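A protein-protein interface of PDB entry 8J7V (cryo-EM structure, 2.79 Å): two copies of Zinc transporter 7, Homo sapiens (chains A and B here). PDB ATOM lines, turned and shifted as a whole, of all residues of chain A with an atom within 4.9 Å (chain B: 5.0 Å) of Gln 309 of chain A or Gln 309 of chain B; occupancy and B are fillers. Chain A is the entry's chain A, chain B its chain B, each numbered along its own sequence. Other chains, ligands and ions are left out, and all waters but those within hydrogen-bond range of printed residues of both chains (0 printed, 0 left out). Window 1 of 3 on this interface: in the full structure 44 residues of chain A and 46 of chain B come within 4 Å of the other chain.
Gln 309 of chain A touches just these residues of chain B: Tyr 112 (3.9 Å), Arg 116 (3.6 Å), Gln 309 (3.6 Å) and Trp 341 (3.2 Å).
Printed residues of chain A within 4 Å of Leu 307 of chain B: Arg 116 (2.8 Å) and Leu 307 (3.9 Å).
Printed residues of chain B within 4 Å of Ser 111 of chain A: Thr 311.
The nearest residue of chain B that does not touch Gln 309 of chain A is Leu 343 of chain B (4.3 Å).
Tyr 112 of chain A touches Trp 341 of chain B (CE2 to CD1, 3.9 Å).
NH1 of Arg 116 of chain A touches NH1 of Arg 116 of chain B, at 3.6 Å.
Met 308 of chain B touches Arg 116 of chain A (SD to C, 3.6 Å).
O of Leu 307 of chain B touches CD2 of Leu 307 of chain A, 3.9 Å away.
Met 308 of chain A touches Arg 116 of chain B (SD to C, 3.7 Å).
Gln 309 of chain A touches Tyr 112 of chain B.
Arg 116 of chain B touches Gln 309 of chain A (NH1 to OE1, 3.6 Å).
Gln 309 of chain A touches Gln 309 of chain B.
NE2 of Gln 309 of chain A touches CH2 of Trp 341 of chain B, at 3.2 Å.
CE2 of Tyr 112 of chain B touches CD1 of Trp 341 of chain A, at 3.9 Å.
OG of Ser 111 of chain A is in hydrogen-bond range of OG1 of Thr 311 of chain B.
The guanidinium group (NH1) of Arg 116 of chain A sits at hydrogen-bond distance from the backbone carbonyl oxygen (O) of Leu 307 of chain B (2.8 Å).
The guanidinium group (NH1) of Arg 116 of chain A lies within hydrogen-bond range of the side-chain amide oxygen (OE1) of Gln 309 of chain B (3.2 Å).
O of Leu 307 of chain A is in hydrogen-bond range of NH1 of Arg 116 of chain B, at 3.0 Å.
The guanidinium group (NH2) of Arg 116 of chain A sits at hydrogen-bond distance from the backbone carbonyl oxygen (O) of Ile 306 of chain A (3.3 Å).
The guanidinium group (NH2) of Arg 116 of chain A sits at hydrogen-bond distance from the side-chain amide oxygen (OE1) of Gln 309 of chain A (2.6 Å).
The backbone carbonyl oxygen of Thr 342 of chain A sits at hydrogen-bond distance from the guanidinium group of Arg 116 of chain A, 2.8 Å away.
NH2 of Arg 116 of chain B is in hydrogen-bond range of OE1 of Gln 309 of chain B, 2.8 Å away.
NH2 of Arg 116 of chain B lies within hydrogen-bond range of O of Thr 342 of chain B.
The guanidinium group (NE) of Arg 116 of chain B sits at hydrogen-bond distance from the backbone carbonyl oxygen (O) of Leu 343 of chain B (2.9 Å).
Ser 111 of chain A touches Thr 311 of chain B, but with the chains exchanged Thr 311 of chain A does not touch Ser 111 of chain B (4.2 Å).
Arg 116 of chain A touches Gln 309 of chain B, and with the chains exchanged Gln 309 of chain A touches Arg 116 of chain B.
Leu 307 of chain A touches its own counterpart, Leu 307 of chain B.
Gln 309 of chain A touches its own counterpart, Gln 309 of chain B.
14 positions are printed for both chains.
Of the 14 printed residues of chain A, 7 touch a printed residue of chain B.
Along chain A the printed residues that touch a printed residue of chain B span positions 111 to 341.
Among the printed residues, 17 pairs touch across the chains.
Among the printed residues, no Asp or Glu carboxylate lies within 4 Å of a Lys or Arg side-chain nitrogen of the other chain.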
ATOM      1  N   SER A 111     -32.480 -18.984 -12.398  1.00  0.00           N
ATOM      2  CA  SER A 111     -31.932 -17.686 -12.778  1.00  0.00           C
ATOM      3  C   SER A 111     -31.347 -17.718 -14.183  1.00  0.00           C
ATOM      4  O   SER A 111     -31.454 -16.740 -14.930  1.00  0.00           O
ATOM      5  CB  SER A 111     -30.869 -17.255 -11.769  1.00  0.00           C
ATOM      6  OG  SER A 111     -31.300 -17.484 -10.443  1.00  0.00           O
ATOM      7  N   TYR A 112     -30.717 -18.825 -14.555  1.00  0.00           N
ATOM      8  CA  TYR A 112     -30.090 -18.953 -15.860  1.00  0.00           C
ATOM      9  C   TYR A 112     -31.058 -19.416 -16.938  1.00  0.00           C
ATOM     10  O   TYR A 112     -30.662 -19.523 -18.100  1.00  0.00           O
ATOM     11  CB  TYR A 112     -28.912 -19.924 -15.779  1.00  0.00           C
ATOM     12  CG  TYR A 112     -27.654 -19.320 -15.201  1.00  0.00           C
ATOM     13  CD1 TYR A 112     -26.875 -18.447 -15.946  1.00  0.00           C
ATOM     14  CD2 TYR A 112     -27.243 -19.630 -13.915  1.00  0.00           C
ATOM     15  CE1 TYR A 112     -25.726 -17.899 -15.423  1.00  0.00           C
ATOM     16  CE2 TYR A 112     -26.094 -19.087 -13.384  1.00  0.00           C
ATOM     17  CZ  TYR A 112     -25.339 -18.220 -14.144  1.00  0.00           C
ATOM     18  OH  TYR A 112     -24.194 -17.671 -13.620  1.00  0.00           O
ATOM     19  N   ARG A 116     -29.996 -25.510 -19.765  1.00  0.00           N
ATOM     20  CA  ARG A 116     -29.259 -26.718 -19.414  1.00  0.00           C
ATOM     21  C   ARG A 116     -30.039 -27.981 -19.741  1.00  0.00           C
ATOM     22  O   ARG A 116     -29.434 -29.052 -19.866  1.00  0.00           O
ATOM     23  CB  ARG A 116     -28.886 -26.698 -17.933  1.00  0.00           C
ATOM     24  CG  ARG A 116     -27.533 -26.079 -17.643  1.00  0.00           C
ATOM     25  CD  ARG A 116     -26.430 -27.113 -17.717  1.00  0.00           C
ATOM     26  NE  ARG A 116     -25.107 -26.517 -17.580  1.00  0.00           N
ATOM     27  CZ  ARG A 116     -24.381 -26.555 -16.472  1.00  0.00           C
ATOM     28  NH1 ARG A 116     -24.820 -27.153 -15.377  1.00  0.00           N
ATOM     29  NH2 ARG A 116     -23.184 -25.980 -16.461  1.00  0.00           N
ATOM     30  N   GLY A 305     -18.231 -32.878 -19.438  1.00  0.00           N
ATOM     31  CA  GLY A 305     -17.442 -31.682 -19.204  1.00  0.00           C
ATOM     32  C   GLY A 305     -18.292 -30.470 -18.873  1.00  0.00           C
ATOM     33  O   GLY A 305     -17.965 -29.703 -17.968  1.00  0.00           O
ATOM     34  N   ILE A 306     -19.396 -30.283 -19.598  1.00  0.00           N
ATOM     35  CA  ILE A 306     -20.266 -29.139 -19.335  1.00  0.00           C
ATOM     36  C   ILE A 306     -20.895 -29.252 -17.952  1.00  0.00           C
ATOM     37  O   ILE A 306     -20.909 -28.292 -17.176  1.00  0.00           O
ATOM     38  CB  ILE A 306     -21.340 -29.007 -20.430  1.00  0.00           C
ATOM     39  CG1 ILE A 306     -20.707 -28.583 -21.753  1.00  0.00           C
ATOM     40  CG2 ILE A 306     -22.386 -27.992 -20.026  1.00  0.00           C
ATOM     41  CD1 ILE A 306     -21.649 -28.667 -22.923  1.00  0.00           C
ATOM     42  N   LEU A 307     -21.410 -30.438 -17.616  1.00  0.00           N
ATOM     43  CA  LEU A 307     -22.101 -30.610 -16.344  1.00  0.00           C
ATOM     44  C   LEU A 307     -21.152 -30.637 -15.151  1.00  0.00           C
ATOM     45  O   LEU A 307     -21.602 -30.429 -14.020  1.00  0.00           O
ATOM     46  CB  LEU A 307     -22.941 -31.885 -16.368  1.00  0.00           C
ATOM     47  CG  LEU A 307     -24.170 -31.852 -17.275  1.00  0.00           C
ATOM     48  CD1 LEU A 307     -24.865 -33.199 -17.290  1.00  0.00           C
ATOM     49  CD2 LEU A 307     -25.123 -30.759 -16.832  1.00  0.00           C
ATOM     50  N   MET A 308     -19.863 -30.883 -15.366  1.00  0.00           N
ATOM     51  CA  MET A 308     -18.883 -30.862 -14.288  1.00  0.00           C
ATOM     52  C   MET A 308     -18.317 -29.472 -14.036  1.00  0.00           C
ATOM     53  O   MET A 308     -17.323 -29.349 -13.312  1.00  0.00           O
ATOM     54  CB  MET A 308     -17.738 -31.834 -14.583  1.00  0.00           C
ATOM     55  CG  MET A 308     -18.075 -33.289 -14.318  1.00  0.00           C
ATOM     56  SD  MET A 308     -17.673 -33.820 -12.650  1.00  0.00           S
ATOM     57  CE  MET A 308     -15.909 -33.546 -12.597  1.00  0.00           C
ATOM     58  N   GLN A 309     -18.924 -28.436 -14.620  1.00  0.00           N
ATOM     59  CA  GLN A 309     -18.482 -27.046 -14.491  1.00  0.00           C
ATOM     60  C   GLN A 309     -17.041 -26.868 -14.955  1.00  0.00           C
ATOM     61  O   GLN A 309     -16.302 -26.040 -14.423  1.00  0.00           O
ATOM     62  CB  GLN A 309     -18.657 -26.533 -13.060  1.00  0.00           C
ATOM     63  CG  GLN A 309     -20.097 -26.505 -12.591  1.00  0.00           C
ATOM     64  CD  GLN A 309     -20.982 -25.652 -13.471  1.00  0.00           C
ATOM     65  OE1 GLN A 309     -21.646 -26.153 -14.372  1.00  0.00           O
ATOM     66  NE2 GLN A 309     -20.999 -24.356 -13.209  1.00  0.00           N
ATOM     67  N   ARG A 310     -16.646 -27.648 -15.955  1.00  0.00           N
ATOM     68  CA  ARG A 310     -15.306 -27.575 -16.514  1.00  0.00           C
ATOM     69  C   ARG A 310     -15.161 -26.328 -17.381  1.00  0.00           C
ATOM     70  O   ARG A 310     -16.141 -25.793 -17.903  1.00  0.00           O
ATOM     71  CB  ARG A 310     -15.023 -28.840 -17.327  1.00  0.00           C
ATOM     72  CG  ARG A 310     -13.632 -28.978 -17.900  1.00  0.00           C
ATOM     73  CD  ARG A 310     -13.629 -29.869 -19.120  1.00  0.00           C
ATOM     74  NE  ARG A 310     -12.279 -30.132 -19.598  1.00  0.00           N
ATOM     75  CZ  ARG A 310     -11.561 -29.281 -20.316  1.00  0.00           C
ATOM     76  NH1 ARG A 310     -12.036 -28.096 -20.664  1.00  0.00           N
ATOM     77  NH2 ARG A 310     -10.337 -29.628 -20.699  1.00  0.00           N
ATOM     78  N   THR A 311     -13.926 -25.855 -17.509  1.00  0.00           N
ATOM     79  CA  THR A 311     -13.634 -24.754 -18.415  1.00  0.00           C
ATOM     80  C   THR A 311     -13.992 -25.161 -19.841  1.00  0.00           C
ATOM     81  O   THR A 311     -13.661 -26.279 -20.257  1.00  0.00           O
ATOM     82  CB  THR A 311     -12.157 -24.369 -18.327  1.00  0.00           C
ATOM     83  OG1 THR A 311     -11.831 -24.031 -16.974  1.00  0.00           O
ATOM     84  CG2 THR A 311     -11.849 -23.180 -19.218  1.00  0.00           C
ATOM     85  N   PHE A 340     -14.422 -20.202 -15.290  1.00  0.00           N
ATOM     86  CA  PHE A 340     -15.150 -20.144 -16.549  1.00  0.00           C
ATOM     87  C   PHE A 340     -15.801 -21.494 -16.793  1.00  0.00           C
ATOM     88  O   PHE A 340     -15.152 -22.533 -16.647  1.00  0.00           O
ATOM     89  CB  PHE A 340     -14.221 -19.757 -17.706  1.00  0.00           C
ATOM     90  CG  PHE A 340     -13.686 -18.360 -17.598  1.00  0.00           C
ATOM     91  CD1 PHE A 340     -12.601 -18.079 -16.786  1.00  0.00           C
ATOM     92  CD2 PHE A 340     -14.281 -17.325 -18.291  1.00  0.00           C
ATOM     93  CE1 PHE A 340     -12.122 -16.795 -16.671  1.00  0.00           C
ATOM     94  CE2 PHE A 340     -13.805 -16.037 -18.179  1.00  0.00           C
ATOM     95  CZ  PHE A 340     -12.725 -15.773 -17.369  1.00  0.00           C
ATOM     96  N   TRP A 341     -17.084 -21.480 -17.135  1.00  0.00           N
ATOM     97  CA  TRP A 341     -17.814 -22.714 -17.381  1.00  0.00           C
ATOM     98  C   TRP A 341     -18.800 -22.504 -18.518  1.00  0.00           C
ATOM     99  O   TRP A 341     -18.980 -21.396 -19.022  1.00  0.00           O
ATOM    100  CB  TRP A 341     -18.535 -23.218 -16.121  1.00  0.00           C
ATOM    101  CG  TRP A 341     -19.294 -22.177 -15.359  1.00  0.00           C
ATOM    102  CD1 TRP A 341     -18.781 -21.252 -14.501  1.00  0.00           C
ATOM    103  CD2 TRP A 341     -20.710 -21.975 -15.364  1.00  0.00           C
ATOM    104  NE1 TRP A 341     -19.786 -20.480 -13.983  1.00  0.00           N
ATOM    105  CE2 TRP A 341     -20.981 -20.904 -14.497  1.00  0.00           C
ATOM    106  CE3 TRP A 341     -21.775 -22.594 -16.025  1.00  0.00           C
ATOM    107  CZ2 TRP A 341     -22.272 -20.438 -14.270  1.00  0.00           C
ATOM    108  CZ3 TRP A 341     -23.055 -22.128 -15.801  1.00  0.00           C
ATOM    109  CH2 TRP A 341     -23.293 -21.061 -14.933  1.00  0.00           C
ATOM    110  N   THR A 342     -19.431 -23.599 -18.927  1.00  0.00           N
ATOM    111  CA  THR A 342     -20.386 -23.607 -20.025  1.00  0.00           C
ATOM    112  C   THR A 342     -21.795 -23.668 -19.455  1.00  0.00           C
ATOM    113  O   THR A 342     -22.115 -24.576 -18.682  1.00  0.00           O
ATOM    114  CB  THR A 342     -20.138 -24.799 -20.947  1.00  0.00           C
ATOM    115  OG1 THR A 342     -18.749 -24.868 -21.288  1.00  0.00           O
ATOM    116  CG2 THR A 342     -20.947 -24.669 -22.208  1.00  0.00           C
ATOM    117  N   LEU A 343     -22.631 -22.704 -19.831  1.00  0.00           N
ATOM    118  CA  LEU A 343     -24.035 -22.759 -19.442  1.00  0.00           C
ATOM    119  C   LEU A 343     -24.817 -23.669 -20.381  1.00  0.00           C
ATOM    120  O   LEU A 343     -25.355 -24.700 -19.965  1.00  0.00           O
ATOM    121  CB  LEU A 343     -24.625 -21.350 -19.435  1.00  0.00           C
ATOM    122  CG  LEU A 343     -26.105 -21.262 -19.094  1.00  0.00           C
ATOM    123  CD1 LEU A 343     -26.318 -21.618 -17.637  1.00  0.00           C
ATOM    124  CD2 LEU A 343     -26.635 -19.879 -19.405  1.00  0.00           C
ATOM    125  N   SER B 111     -11.642 -25.833 -12.952  1.00  0.00           N
ATOM    126  CA  SER B 111     -11.346 -24.758 -12.013  1.00  0.00           C
ATOM    127  C   SER B 111     -12.095 -24.931 -10.701  1.00  0.00           C
ATOM    128  O   SER B 111     -11.632 -24.455  -9.659  1.00  0.00           O
ATOM    129  CB  SER B 111     -11.685 -23.408 -12.641  1.00  0.00           C
ATOM    130  OG  SER B 111     -13.037 -23.366 -13.058  1.00  0.00           O
ATOM    131  N   TYR B 112     -13.243 -25.596 -10.729  1.00  0.00           N
ATOM    132  CA  TYR B 112     -14.070 -25.791  -9.549  1.00  0.00           C
ATOM    133  C   TYR B 112     -13.784 -27.106  -8.845  1.00  0.00           C
ATOM    134  O   TYR B 112     -14.480 -27.445  -7.885  1.00  0.00           O
ATOM    135  CB  TYR B 112     -15.549 -25.729  -9.929  1.00  0.00           C
ATOM    136  CG  TYR B 112     -16.112 -24.335 -10.018  1.00  0.00           C
ATOM    137  CD1 TYR B 112     -16.384 -23.602  -8.874  1.00  0.00           C
ATOM    138  CD2 TYR B 112     -16.384 -23.755 -11.246  1.00  0.00           C
ATOM    139  CE1 TYR B 112     -16.903 -22.330  -8.952  1.00  0.00           C
ATOM    140  CE2 TYR B 112     -16.907 -22.487 -11.332  1.00  0.00           C
ATOM    141  CZ  TYR B 112     -17.161 -21.777 -10.182  1.00  0.00           C
ATOM    142  OH  TYR B 112     -17.679 -20.507 -10.256  1.00  0.00           O
ATOM    143  N   ARG B 116     -18.397 -31.958  -8.663  1.00  0.00           N
ATOM    144  CA  ARG B 116     -19.637 -32.227  -9.386  1.00  0.00           C
ATOM    145  C   ARG B 116     -19.821 -33.703  -9.701  1.00  0.00           C
ATOM    146  O   ARG B 116     -20.965 -34.151  -9.849  1.00  0.00           O
ATOM    147  CB  ARG B 116     -19.675 -31.422 -10.685  1.00  0.00           C
ATOM    148  CG  ARG B 116     -20.302 -30.049 -10.563  1.00  0.00           C
ATOM    149  CD  ARG B 116     -21.812 -30.130 -10.526  1.00  0.00           C
ATOM    150  NE  ARG B 116     -22.414 -28.827 -10.277  1.00  0.00           N
ATOM    151  CZ  ARG B 116     -23.099 -28.133 -11.175  1.00  0.00           C
ATOM    152  NH1 ARG B 116     -23.304 -28.594 -12.397  1.00  0.00           N
ATOM    153  NH2 ARG B 116     -23.591 -26.945 -10.839  1.00  0.00           N
ATOM    154  N   GLY B 305     -32.033 -30.618 -10.380  1.00  0.00           N
ATOM    155  CA  GLY B 305     -32.017 -29.246  -9.906  1.00  0.00           C
ATOM    156  C   GLY B 305     -30.617 -28.674  -9.820  1.00  0.00           C
ATOM    157  O   GLY B 305     -30.377 -27.537 -10.229  1.00  0.00           O
ATOM    158  N   ILE B 306     -29.670 -29.455  -9.297  1.00  0.00           N
ATOM    159  CA  ILE B 306     -28.292 -28.970  -9.218  1.00  0.00           C
ATOM    160  C   ILE B 306     -27.710 -28.774 -10.615  1.00  0.00           C
ATOM    161  O   ILE B 306     -27.125 -27.728 -10.920  1.00  0.00           O
ATOM    162  CB  ILE B 306     -27.427 -29.918  -8.371  1.00  0.00           C
ATOM    163  CG1 ILE B 306     -27.684 -29.672  -6.888  1.00  0.00           C
ATOM    164  CG2 ILE B 306     -25.957 -29.713  -8.677  1.00  0.00           C
ATOM    165  CD1 ILE B 306     -27.045 -30.681  -5.989  1.00  0.00           C
ATOM    166  N   LEU B 307     -27.884 -29.765 -11.490  1.00  0.00           N
ATOM    167  CA  LEU B 307     -27.268 -29.716 -12.812  1.00  0.00           C
ATOM    168  C   LEU B 307     -27.897 -28.678 -13.729  1.00  0.00           C
ATOM    169  O   LEU B 307     -27.270 -28.291 -14.718  1.00  0.00           O
ATOM    170  CB  LEU B 307     -27.333 -31.092 -13.471  1.00  0.00           C
ATOM    171  CG  LEU B 307     -26.486 -32.169 -12.798  1.00  0.00           C
ATOM    172  CD1 LEU B 307     -26.611 -33.495 -13.527  1.00  0.00           C
ATOM    173  CD2 LEU B 307     -25.040 -31.721 -12.720  1.00  0.00           C
ATOM    174  N   MET B 308     -29.110 -28.218 -13.432  1.00  0.00           N
ATOM    175  CA  MET B 308     -29.778 -27.216 -14.251  1.00  0.00           C
ATOM    176  C   MET B 308     -29.445 -25.792 -13.830  1.00  0.00           C
ATOM    177  O   MET B 308     -30.101 -24.857 -14.297  1.00  0.00           O
ATOM    178  CB  MET B 308     -31.294 -27.424 -14.214  1.00  0.00           C
ATOM    179  CG  MET B 308     -31.791 -28.605 -15.040  1.00  0.00           C
ATOM    180  SD  MET B 308     -31.997 -28.245 -16.790  1.00  0.00           S
ATOM    181  CE  MET B 308     -33.262 -26.982 -16.731  1.00  0.00           C
ATOM    182  N   GLN B 309     -28.441 -25.616 -12.964  1.00  0.00           N
ATOM    183  CA  GLN B 309     -28.029 -24.308 -12.443  1.00  0.00           C
ATOM    184  C   GLN B 309     -29.186 -23.594 -11.750  1.00  0.00           C
ATOM    185  O   GLN B 309     -29.333 -22.375 -11.835  1.00  0.00           O
ATOM    186  CB  GLN B 309     -27.422 -23.431 -13.540  1.00  0.00           C
ATOM    187  CG  GLN B 309     -26.177 -24.022 -14.175  1.00  0.00           C
ATOM    188  CD  GLN B 309     -25.073 -24.283 -13.171  1.00  0.00           C
ATOM    189  OE1 GLN B 309     -24.868 -25.412 -12.737  1.00  0.00           O
ATOM    190  NE2 GLN B 309     -24.352 -23.238 -12.802  1.00  0.00           N
ATOM    191  N   ARG B 310     -30.012 -24.365 -11.056  1.00  0.00           N
ATOM    192  CA  ARG B 310     -31.145 -23.821 -10.333  1.00  0.00           C
ATOM    193  C   ARG B 310     -30.677 -23.154  -9.045  1.00  0.00           C
ATOM    194  O   ARG B 310     -29.633 -23.498  -8.487  1.00  0.00           O
ATOM    195  CB  ARG B 310     -32.149 -24.935 -10.037  1.00  0.00           C
ATOM    196  CG  ARG B 310     -33.479 -24.491  -9.479  1.00  0.00           C
ATOM    197  CD  ARG B 310     -34.007 -25.504  -8.489  1.00  0.00           C
ATOM    198  NE  ARG B 310     -35.343 -25.165  -8.021  1.00  0.00           N
ATOM    199  CZ  ARG B 310     -35.595 -24.324  -7.029  1.00  0.00           C
ATOM    200  NH1 ARG B 310     -34.620 -23.717  -6.374  1.00  0.00           N
ATOM    201  NH2 ARG B 310     -36.856 -24.088  -6.684  1.00  0.00           N
ATOM    202  N   THR B 311     -31.449 -22.174  -8.590  1.00  0.00           N
ATOM    203  CA  THR B 311     -31.176 -21.545  -7.307  1.00  0.00           C
ATOM    204  C   THR B 311     -31.301 -22.591  -6.205  1.00  0.00           C
ATOM    205  O   THR B 311     -32.268 -23.364  -6.204  1.00  0.00           O
ATOM    206  CB  THR B 311     -32.147 -20.388  -7.066  1.00  0.00           C
ATOM    207  OG1 THR B 311     -31.879 -19.336  -8.000  1.00  0.00           O
ATOM    208  CG2 THR B 311     -32.011 -19.837  -5.659  1.00  0.00           C
ATOM    209  N   PHE B 340     -27.534 -17.530  -8.631  1.00  0.00           N
ATOM    210  CA  PHE B 340     -27.097 -18.396  -7.548  1.00  0.00           C
ATOM    211  C   PHE B 340     -27.306 -19.845  -7.950  1.00  0.00           C
ATOM    212  O   PHE B 340     -28.322 -20.185  -8.561  1.00  0.00           O
ATOM    213  CB  PHE B 340     -27.850 -18.094  -6.252  1.00  0.00           C
ATOM    214  CG  PHE B 340     -27.485 -16.778  -5.645  1.00  0.00           C
ATOM    215  CD1 PHE B 340     -28.173 -15.631  -5.988  1.00  0.00           C
ATOM    216  CD2 PHE B 340     -26.451 -16.687  -4.739  1.00  0.00           C
ATOM    217  CE1 PHE B 340     -27.834 -14.422  -5.440  1.00  0.00           C
ATOM    218  CE2 PHE B 340     -26.106 -15.480  -4.190  1.00  0.00           C
ATOM    219  CZ  PHE B 340     -26.799 -14.346  -4.541  1.00  0.00           C
ATOM    220  N   TRP B 341     -26.342 -20.696  -7.613  1.00  0.00           N
ATOM    221  CA  TRP B 341     -26.458 -22.102  -7.969  1.00  0.00           C
ATOM    222  C   TRP B 341     -25.664 -22.948  -6.987  1.00  0.00           C
ATOM    223  O   TRP B 341     -24.868 -22.447  -6.194  1.00  0.00           O
ATOM    224  CB  TRP B 341     -26.000 -22.369  -9.407  1.00  0.00           C
ATOM    225  CG  TRP B 341     -24.685 -21.761  -9.786  1.00  0.00           C
ATOM    226  CD1 TRP B 341     -24.452 -20.468 -10.142  1.00  0.00           C
ATOM    227  CD2 TRP B 341     -23.424 -22.433  -9.873  1.00  0.00           C
ATOM    228  NE1 TRP B 341     -23.126 -20.289 -10.436  1.00  0.00           N
ATOM    229  CE2 TRP B 341     -22.473 -21.481 -10.281  1.00  0.00           C
ATOM    230  CE3 TRP B 341     -23.009 -23.747  -9.642  1.00  0.00           C
ATOM    231  CZ2 TRP B 341     -21.130 -21.802 -10.463  1.00  0.00           C
ATOM    232  CZ3 TRP B 341     -21.679 -24.062  -9.821  1.00  0.00           C
ATOM    233  CH2 TRP B 341     -20.754 -23.094 -10.227  1.00  0.00           C
ATOM    234  N   THR B 342     -25.915 -24.250  -7.048  1.00  0.00           N
ATOM    235  CA  THR B 342     -25.271 -25.231  -6.188  1.00  0.00           C
ATOM    236  C   THR B 342     -24.105 -25.856  -6.940  1.00  0.00           C
ATOM    237  O   THR B 342     -24.297 -26.441  -8.010  1.00  0.00           O
ATOM    238  CB  THR B 342     -26.270 -26.309  -5.771  1.00  0.00           C
ATOM    239  OG1 THR B 342     -27.562 -25.722  -5.586  1.00  0.00           O
ATOM    240  CG2 THR B 342     -25.841 -26.956  -4.485  1.00  0.00           C
ATOM    241  N   LEU B 343     -22.901 -25.730  -6.382  1.00  0.00           N
ATOM    242  CA  LEU B 343     -21.746 -26.408  -6.961  1.00  0.00           C
ATOM    243  C   LEU B 343     -21.728 -27.878  -6.567  1.00  0.00           C
ATOM    244  O   LEU B 343     -21.691 -28.764  -7.426  1.00  0.00           O
ATOM    245  CB  LEU B 343     -20.459 -25.715  -6.519  1.00  0.00           C
ATOM    246  CG  LEU B 343     -19.165 -26.372  -6.991  1.00  0.00           C
ATOM    247  CD1 LEU B 343     -18.979 -26.160  -8.480  1.00  0.00           C
ATOM    248  CD2 LEU B 343     -17.986 -25.835  -6.214  1.00  0.00           C
